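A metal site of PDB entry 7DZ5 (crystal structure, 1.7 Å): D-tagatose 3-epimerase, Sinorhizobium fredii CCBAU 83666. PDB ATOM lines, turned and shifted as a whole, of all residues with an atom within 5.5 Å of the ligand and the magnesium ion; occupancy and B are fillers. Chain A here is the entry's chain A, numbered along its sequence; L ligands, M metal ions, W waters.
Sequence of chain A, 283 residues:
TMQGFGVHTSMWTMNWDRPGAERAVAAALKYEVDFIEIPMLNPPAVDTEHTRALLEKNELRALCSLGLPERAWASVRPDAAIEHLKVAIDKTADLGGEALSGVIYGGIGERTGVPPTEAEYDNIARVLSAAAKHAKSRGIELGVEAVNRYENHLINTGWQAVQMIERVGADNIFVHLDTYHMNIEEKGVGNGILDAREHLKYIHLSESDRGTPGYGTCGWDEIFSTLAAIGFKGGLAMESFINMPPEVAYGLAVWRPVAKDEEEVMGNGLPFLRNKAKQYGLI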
ATOM      1  N   HIS A   8     -29.646  24.699  10.633  1.00  0.00           N
ATOM      2  CA  HIS A   8     -29.240  23.945   9.461  1.00  0.00           C
ATOM      3  C   HIS A   8     -29.838  24.633   8.230  1.00  0.00           C
ATOM      4  O   HIS A   8     -31.050  24.896   8.190  1.00  0.00           O
ATOM      5  CB  HIS A   8     -29.719  22.502   9.574  1.00  0.00           C
ATOM      6  CG  HIS A   8     -29.190  21.617   8.496  1.00  0.00           C
ATOM      7  ND1 HIS A   8     -29.306  21.926   7.161  1.00  0.00           N
ATOM      8  CD2 HIS A   8     -28.558  20.424   8.550  1.00  0.00           C
ATOM      9  CE1 HIS A   8     -28.740  20.980   6.438  1.00  0.00           C
ATOM     10  NE2 HIS A   8     -28.276  20.050   7.265  1.00  0.00           N
ATOM     11  N   MET A  14     -29.709  23.466   0.019  1.00  0.00           N
ATOM     12  CA  MET A  14     -28.961  22.215   0.130  1.00  0.00           C
ATOM     13  C   MET A  14     -27.830  22.102  -0.871  1.00  0.00           C
ATOM     14  O   MET A  14     -26.951  21.257  -0.685  1.00  0.00           O
ATOM     15  CB  MET A  14     -29.873  20.986  -0.093  1.00  0.00           C
ATOM     16  CG  MET A  14     -30.887  20.749   0.988  1.00  0.00           C
ATOM     17  SD  MET A  14     -30.072  20.293   2.522  1.00  0.00           S
ATOM     18  CE  MET A  14     -29.187  18.767   2.172  1.00  0.00           C
ATOM     19  N   GLU A  37     -25.148  25.696   9.964  1.00  0.00           N
ATOM     20  CA  GLU A  37     -24.666  24.378   9.581  1.00  0.00           C
ATOM     21  C   GLU A  37     -24.829  24.261   8.073  1.00  0.00           C
ATOM     22  O   GLU A  37     -25.950  24.374   7.558  1.00  0.00           O
ATOM     23  CB  GLU A  37     -25.445  23.279  10.295  1.00  0.00           C
ATOM     24  CG  GLU A  37     -25.053  21.909   9.876  1.00  0.00           C
ATOM     25  CD  GLU A  37     -25.919  20.873  10.576  1.00  0.00           C
ATOM     26  OE1 GLU A  37     -26.542  21.249  11.597  1.00  0.00           O
ATOM     27  OE2 GLU A  37     -25.979  19.712  10.091  1.00  0.00           O
ATOM     28  N   PRO A  39     -24.749  22.191   4.652  1.00  0.00           N
ATOM     29  CA  PRO A  39     -24.771  20.845   4.076  1.00  0.00           C
ATOM     30  C   PRO A  39     -23.795  20.731   2.912  1.00  0.00           C
ATOM     31  O   PRO A  39     -23.709  21.629   2.066  1.00  0.00           O
ATOM     32  CB  PRO A  39     -26.212  20.675   3.596  1.00  0.00           C
ATOM     33  CG  PRO A  39     -26.638  22.076   3.265  1.00  0.00           C
ATOM     34  CD  PRO A  39     -25.912  22.990   4.253  1.00  0.00           C
ATOM     35  N   MET A  40     -23.087  19.614   2.865  1.00  0.00           N
ATOM     36  CA  MET A  40     -22.099  19.349   1.811  1.00  0.00           C
ATOM     37  C   MET A  40     -22.492  18.103   1.030  1.00  0.00           C
ATOM     38  O   MET A  40     -21.922  17.025   1.243  1.00  0.00           O
ATOM     39  CB  MET A  40     -20.781  19.239   2.415  1.00  0.00           C
ATOM     40  CG  MET A  40     -20.374  20.530   3.116  1.00  0.00           C
ATOM     41  SD  MET A  40     -18.721  21.134   2.723  1.00  0.00           S
ATOM     42  CE  MET A  40     -17.968  19.574   2.725  1.00  0.00           C
ATOM     43  N   SER A  65     -21.945  19.513   7.509  1.00  0.00           N
ATOM     44  CA  SER A  65     -22.475  18.174   7.752  1.00  0.00           C
ATOM     45  C   SER A  65     -22.773  17.473   6.438  1.00  0.00           C
ATOM     46  O   SER A  65     -22.959  18.107   5.396  1.00  0.00           O
ATOM     47  CB  SER A  65     -23.735  18.208   8.641  1.00  0.00           C
ATOM     48  OG  SER A  65     -24.762  18.927   7.987  1.00  0.00           O
ATOM     49  N   LEU A  66     -22.796  16.149   6.495  1.00  0.00           N
ATOM     50  CA  LEU A  66     -23.053  15.322   5.336  1.00  0.00           C
ATOM     51  C   LEU A  66     -23.462  13.933   5.804  1.00  0.00           C
ATOM     52  O   LEU A  66     -23.352  13.591   6.991  1.00  0.00           O
ATOM     53  CB  LEU A  66     -21.834  15.221   4.407  1.00  0.00           C
ATOM     54  CG  LEU A  66     -20.550  14.572   4.934  1.00  0.00           C
ATOM     55  CD1 LEU A  66     -20.620  13.028   4.998  1.00  0.00           C
ATOM     56  CD2 LEU A  66     -19.347  14.987   4.069  1.00  0.00           C
ATOM     57  N   GLY A  67     -23.965  13.162   4.853  1.00  0.00           N
ATOM     58  CA  GLY A  67     -24.034  11.712   4.966  1.00  0.00           C
ATOM     59  C   GLY A  67     -23.274  11.077   3.811  1.00  0.00           C
ATOM     60  O   GLY A  67     -23.230  11.626   2.710  1.00  0.00           O
ATOM     61  N   SER A 101     -19.851  17.200  10.716  1.00  0.00           N
ATOM     62  CA  SER A 101     -20.717  16.335  11.533  1.00  0.00           C
ATOM     63  C   SER A 101     -21.758  15.682  10.633  1.00  0.00           C
ATOM     64  O   SER A 101     -21.684  15.753   9.401  1.00  0.00           O
ATOM     65  CB  SER A 101     -21.341  17.143  12.680  1.00  0.00           C
ATOM     66  OG  SER A 101     -21.861  16.319  13.703  1.00  0.00           O
ATOM     67  N   GLY A 102     -22.652  14.934  11.245  1.00  0.00           N
ATOM     68  CA  GLY A 102     -23.680  14.242  10.500  1.00  0.00           C
ATOM     69  C   GLY A 102     -23.455  12.755  10.463  1.00  0.00           C
ATOM     70  O   GLY A 102     -22.853  12.163  11.381  1.00  0.00           O
ATOM     71  N   VAL A 103     -23.939  12.122   9.397  1.00  0.00           N
ATOM     72  CA  VAL A 103     -23.829  10.672   9.247  1.00  0.00           C
ATOM     73  C   VAL A 103     -22.500  10.436   8.510  1.00  0.00           C
ATOM     74  O   VAL A 103     -22.483  10.052   7.341  1.00  0.00           O
ATOM     75  CB  VAL A 103     -25.054  10.088   8.510  1.00  0.00           C
ATOM     76  CG1 VAL A 103     -25.000   8.579   8.509  1.00  0.00           C
ATOM     77  CG2 VAL A 103     -26.352  10.561   9.169  1.00  0.00           C
ATOM     78  N   ILE A 108     -27.506   7.282   4.711  1.00  0.00           N
ATOM     79  CA  ILE A 108     -28.944   7.111   4.743  1.00  0.00           C
ATOM     80  C   ILE A 108     -29.315   6.017   3.745  1.00  0.00           C
ATOM     81  O   ILE A 108     -28.924   6.065   2.572  1.00  0.00           O
ATOM     82  CB  ILE A 108     -29.643   8.449   4.441  1.00  0.00           C
ATOM     83  CG1 ILE A 108     -29.119   9.563   5.370  1.00  0.00           C
ATOM     84  CG2 ILE A 108     -31.172   8.269   4.496  1.00  0.00           C
ATOM     85  CD1 ILE A 108     -29.257   9.320   6.879  1.00  0.00           C
ATOM     86  N   GLU A 145     -23.519  11.819  14.218  1.00  0.00           N
ATOM     87  CA  GLU A 145     -24.944  12.013  14.487  1.00  0.00           C
ATOM     88  C   GLU A 145     -25.648  10.670  14.526  1.00  0.00           C
ATOM     89  O   GLU A 145     -25.667   9.936  13.529  1.00  0.00           O
ATOM     90  CB  GLU A 145     -25.612  12.913  13.442  1.00  0.00           C
ATOM     91  CG  GLU A 145     -27.094  13.218  13.744  1.00  0.00           C
ATOM     92  CD  GLU A 145     -27.751  14.209  12.772  1.00  0.00           C
ATOM     93  OE1 GLU A 145     -27.095  14.612  11.781  1.00  0.00           O
ATOM     94  OE2 GLU A 145     -28.918  14.600  12.995  1.00  0.00           O
ATOM     95  N   VAL A 147     -28.807   8.515  14.195  1.00  0.00           N
ATOM     96  CA  VAL A 147     -30.047   8.668  13.427  1.00  0.00           C
ATOM     97  C   VAL A 147     -30.904   7.421  13.650  1.00  0.00           C
ATOM     98  O   VAL A 147     -30.432   6.401  14.149  1.00  0.00           O
ATOM     99  CB  VAL A 147     -29.800   8.911  11.932  1.00  0.00           C
ATOM    100  CG1 VAL A 147     -28.982  10.217  11.750  1.00  0.00           C
ATOM    101  CG2 VAL A 147     -29.104   7.732  11.288  1.00  0.00           C
ATOM    102  N   GLU A 151     -33.020   4.836   8.964  1.00  0.00           N
ATOM    103  CA  GLU A 151     -32.078   5.545   8.111  1.00  0.00           C
ATOM    104  C   GLU A 151     -30.738   4.845   8.082  1.00  0.00           C
ATOM    105  O   GLU A 151     -30.041   4.878   7.049  1.00  0.00           O
ATOM    106  CB  GLU A 151     -31.940   6.979   8.593  1.00  0.00           C
ATOM    107  CG  GLU A 151     -33.239   7.756   8.348  1.00  0.00           C
ATOM    108  CD  GLU A 151     -33.128   9.263   8.535  1.00  0.00           C
ATOM    109  OE1 GLU A 151     -32.005   9.804   8.656  1.00  0.00           O
ATOM    110  OE2 GLU A 151     -34.201   9.897   8.562  1.00  0.00           O
ATOM    111  N   HIS A 176     -23.345  14.058  18.264  1.00  0.00           N
ATOM    112  CA  HIS A 176     -24.319  14.965  17.690  1.00  0.00           C
ATOM    113  C   HIS A 176     -25.657  14.237  17.816  1.00  0.00           C
ATOM    114  O   HIS A 176     -25.803  13.143  17.271  1.00  0.00           O
ATOM    115  CB  HIS A 176     -23.892  15.242  16.250  1.00  0.00           C
ATOM    116  CG  HIS A 176     -24.871  15.994  15.403  1.00  0.00           C
ATOM    117  ND1 HIS A 176     -24.524  16.500  14.164  1.00  0.00           N
ATOM    118  CD2 HIS A 176     -26.189  16.270  15.559  1.00  0.00           C
ATOM    119  CE1 HIS A 176     -25.568  17.091  13.621  1.00  0.00           C
ATOM    120  NE2 HIS A 176     -26.590  16.972  14.444  1.00  0.00           N
ATOM    121  N   ASP A 178     -30.066  14.348  17.742  1.00  0.00           N
ATOM    122  CA  ASP A 178     -31.152  14.960  16.966  1.00  0.00           C
ATOM    123  C   ASP A 178     -32.468  14.561  17.631  1.00  0.00           C
ATOM    124  O   ASP A 178     -32.770  13.375  17.768  1.00  0.00           O
ATOM    125  CB  ASP A 178     -31.068  14.485  15.501  1.00  0.00           C
ATOM    126  CG  ASP A 178     -32.150  15.087  14.611  1.00  0.00           C
ATOM    127  OD1 ASP A 178     -33.303  15.151  15.021  1.00  0.00           O
ATOM    128  OD2 ASP A 178     -31.851  15.393  13.435  1.00  0.00           O
ATOM    129  N   TYR A 180     -35.518  14.652  16.718  1.00  0.00           N
ATOM    130  CA  TYR A 180     -36.406  13.838  15.893  1.00  0.00           C
ATOM    131  C   TYR A 180     -36.024  12.359  15.952  1.00  0.00           C
ATOM    132  O   TYR A 180     -36.896  11.489  16.066  1.00  0.00           O
ATOM    133  CB  TYR A 180     -36.363  14.337  14.458  1.00  0.00           C
ATOM    134  CG  TYR A 180     -36.926  13.422  13.399  1.00  0.00           C
ATOM    135  CD1 TYR A 180     -38.253  13.493  13.034  1.00  0.00           C
ATOM    136  CD2 TYR A 180     -36.100  12.532  12.714  1.00  0.00           C
ATOM    137  CE1 TYR A 180     -38.754  12.707  12.014  1.00  0.00           C
ATOM    138  CE2 TYR A 180     -36.602  11.718  11.705  1.00  0.00           C
ATOM    139  CZ  TYR A 180     -37.929  11.822  11.370  1.00  0.00           C
ATOM    140  OH  TYR A 180     -38.430  11.040  10.359  1.00  0.00           O
ATOM    141  N   HIS A 181     -34.729  12.071  15.875  1.00  0.00           N
ATOM    142  CA  HIS A 181     -34.274  10.678  15.946  1.00  0.00           C
ATOM    143  C   HIS A 181     -34.398  10.147  17.371  1.00  0.00           C
ATOM    144  O   HIS A 181     -34.821   8.999  17.566  1.00  0.00           O
ATOM    145  CB  HIS A 181     -32.839  10.570  15.452  1.00  0.00           C
ATOM    146  CG  HIS A 181     -32.690  10.894  13.989  1.00  0.00           C
ATOM    147  ND1 HIS A 181     -33.408  10.249  13.008  1.00  0.00           N
ATOM    148  CD2 HIS A 181     -31.930  11.813  13.363  1.00  0.00           C
ATOM    149  CE1 HIS A 181     -33.092  10.758  11.831  1.00  0.00           C
ATOM    150  NE2 HIS A 181     -32.178  11.707  12.019  1.00  0.00           N
ATOM    151  N   HIS A 204     -29.386  18.760  17.078  1.00  0.00           N
ATOM    152  CA  HIS A 204     -30.453  19.213  16.191  1.00  0.00           C
ATOM    153  C   HIS A 204     -31.769  19.266  16.954  1.00  0.00           C
ATOM    154  O   HIS A 204     -32.209  18.248  17.496  1.00  0.00           O
ATOM    155  CB  HIS A 204     -30.593  18.264  15.005  1.00  0.00           C
ATOM    156  CG  HIS A 204     -29.655  18.590  13.900  1.00  0.00           C
ATOM    157  ND1 HIS A 204     -29.368  17.716  12.877  1.00  0.00           N
ATOM    158  CD2 HIS A 204     -28.913  19.705  13.681  1.00  0.00           C
ATOM    159  CE1 HIS A 204     -28.501  18.289  12.052  1.00  0.00           C
ATOM    160  NE2 HIS A 204     -28.210  19.486  12.518  1.00  0.00           N
ATOM    161  N   ARG A 210     -40.572  16.588  11.612  1.00  0.00           N
ATOM    162  CA  ARG A 210     -39.668  17.476  10.862  1.00  0.00           C
ATOM    163  C   ARG A 210     -40.316  18.818  10.517  1.00  0.00           C
ATOM    164  O   ARG A 210     -39.795  19.550   9.678  1.00  0.00           O
ATOM    165  CB  ARG A 210     -39.155  16.826   9.579  1.00  0.00           C
ATOM    166  CG  ARG A 210     -38.292  15.569   9.833  1.00  0.00           C
ATOM    167  CD  ARG A 210     -37.067  15.903  10.642  1.00  0.00           C
ATOM    168  NE  ARG A 210     -36.000  14.931  10.452  1.00  0.00           N
ATOM    169  CZ  ARG A 210     -34.795  15.026  11.020  1.00  0.00           C
ATOM    170  NH1 ARG A 210     -34.510  16.040  11.822  1.00  0.00           N
ATOM    171  NH2 ARG A 210     -33.863  14.113  10.741  1.00  0.00           N
ATOM    172  N   GLU A 239     -33.484  22.370  13.076  1.00  0.00           N
ATOM    173  CA  GLU A 239     -33.536  21.615  11.819  1.00  0.00           C
ATOM    174  C   GLU A 239     -34.993  21.364  11.464  1.00  0.00           C
ATOM    175  O   GLU A 239     -35.748  20.829  12.289  1.00  0.00           O
ATOM    176  CB  GLU A 239     -32.749  20.288  11.905  1.00  0.00           C
ATOM    177  CG  GLU A 239     -32.863  19.404  10.610  1.00  0.00           C
ATOM    178  CD  GLU A 239     -31.845  18.273  10.532  1.00  0.00           C
ATOM    179  OE1 GLU A 239     -31.892  17.313  11.360  1.00  0.00           O
ATOM    180  OE2 GLU A 239     -31.002  18.296   9.603  1.00  0.00           O
ATOM    181  N   PHE A 241     -37.474  20.346   7.786  1.00  0.00           N
ATOM    182  CA  PHE A 241     -37.409  19.959   6.384  1.00  0.00           C
ATOM    183  C   PHE A 241     -38.334  20.809   5.491  1.00  0.00           C
ATOM    184  O   PHE A 241     -38.515  20.473   4.310  1.00  0.00           O
ATOM    185  CB  PHE A 241     -37.721  18.476   6.238  1.00  0.00           C
ATOM    186  CG  PHE A 241     -36.603  17.567   6.709  1.00  0.00           C
ATOM    187  CD1 PHE A 241     -35.402  18.070   7.167  1.00  0.00           C
ATOM    188  CD2 PHE A 241     -36.776  16.205   6.702  1.00  0.00           C
ATOM    189  CE1 PHE A 241     -34.392  17.224   7.622  1.00  0.00           C
ATOM    190  CE2 PHE A 241     -35.775  15.365   7.145  1.00  0.00           C
ATOM    191  CZ  PHE A 241     -34.583  15.877   7.599  1.00  0.00           C
ATOM    192  N   LEU A 252     -35.212  11.334   2.418  1.00  0.00           N
ATOM    193  CA  LEU A 252     -35.460  11.348   3.859  1.00  0.00           C
ATOM    194  C   LEU A 252     -36.894  10.986   4.209  1.00  0.00           C
ATOM    195  O   LEU A 252     -37.345  11.224   5.338  1.00  0.00           O
ATOM    196  CB  LEU A 252     -35.106  12.718   4.423  1.00  0.00           C
ATOM    197  CG  LEU A 252     -33.593  12.976   4.317  1.00  0.00           C
ATOM    198  CD1 LEU A 252     -33.286  14.460   4.323  1.00  0.00           C
ATOM    199  CD2 LEU A 252     -32.862  12.258   5.455  1.00  0.00           C
HETATM  200  C1  LIG L   1     -30.763  12.910   8.824  1.00  0.00           C
HETATM  201  O1  LIG L   1     -31.814  12.157   9.318  1.00  0.00           O
HETATM  202  C2  LIG L   1     -30.301  13.994   9.807  1.00  0.00           C
HETATM  203  O2  LIG L   1     -30.929  14.208  10.823  1.00  0.00           O
HETATM  204  C3  LIG L   1     -29.004  14.766   9.450  1.00  0.00           C
HETATM  205  O3  LIG L   1     -28.847  15.882  10.285  1.00  0.00           O
HETATM  206  C4  LIG L   1     -29.072  15.165   7.964  1.00  0.00           C
HETATM  207  O4  LIG L   1     -30.039  16.185   7.893  1.00  0.00           O
HETATM  208  C5  LIG L   1     -27.727  15.541   7.298  1.00  0.00           C
HETATM  209  O5  LIG L   1     -26.672  15.666   8.214  1.00  0.00           O
HETATM  210  C6  LIG L   1     -27.889  16.788   6.412  1.00  0.00           C
HETATM  211  O6  LIG L   1     -26.679  17.512   6.231  1.00  0.00           O
HETATM  212 MG    MG M   1     -30.343  15.828  12.142  1.00  0.00          MG
HETATM  213  O   HOH W   1     -25.974  16.953   3.498  1.00  0.00           O
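OE1 of Glu 151 is in hydrogen-bond range of O1 of the ligand.
An oxygen (O1) of the ligand lies within hydrogen-bond range of a ring nitrogen (NE2) of His 181 (2.8 Å).
NH2 of Arg 210 lies within hydrogen-bond range of O1 of the ligand (3.2 Å).
An oxygen (O6) of the ligand is in hydrogen-bond range of the side-chain hydroxyl (OG) of Ser 65, at 3.0 Å.
NE2 of His 8 is in hydrogen-bond range of O6 of the ligand, 3.2 Å away.
N of Glu 145 sits at hydrogen-bond distance from O of Gly 102 (2.9 Å).
The side-chain carboxylate (OE1) of Glu 37 sits at hydrogen-bond distance from a ring nitrogen (NE2) of His 204, 2.6 Å away.
ND1 of His 204 sits close to NE2 of His 176 (3.3 Å).
The side-chain carboxylate (OE1) of Glu 239 sits close to the guanidinium group (NH1) of Arg 210, at 2.9 Å.
NH2 of Arg 210 is in hydrogen-bond range of NE2 of His 181, at 3.2 Å.
The backbone carbonyl oxygen (O) of Arg 210 is in hydrogen-bond range of the backbone NH (N) of Phe 241, at 3.1 Å.
The side-chain hydroxyl of Ser 65 is in hydrogen-bond range of the side-chain carboxylate of Glu 37 (2.6 Å).
O of Ser 65 sits at hydrogen-bond distance from N of Met 40, at 2.9 Å.
Hydrophobic or aromatic side chains that line the ligand: His 181 and His 204.
Of the 24 residues printed, 4 come within 4 Å of the magnesium ion.
The nearest printed residue that does not touch the magnesium ion is Arg 210 (4.2 Å).
The magnesium ion is bound by OD2 of Asp 178 (2.0 Å).
The magnesium ion is bound by OE2 of Glu 145 (2.1 Å).
O2 of the ligand binds the magnesium ion, 2.2 Å away.
ND1 of His 204 is bound to the magnesium ion, 2.2 Å away.
OE1 of Glu 239 is bound to the magnesium ion, at 2.3 Å.
The magnesium ion is bound by O3 of the ligand (2.4 Å).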
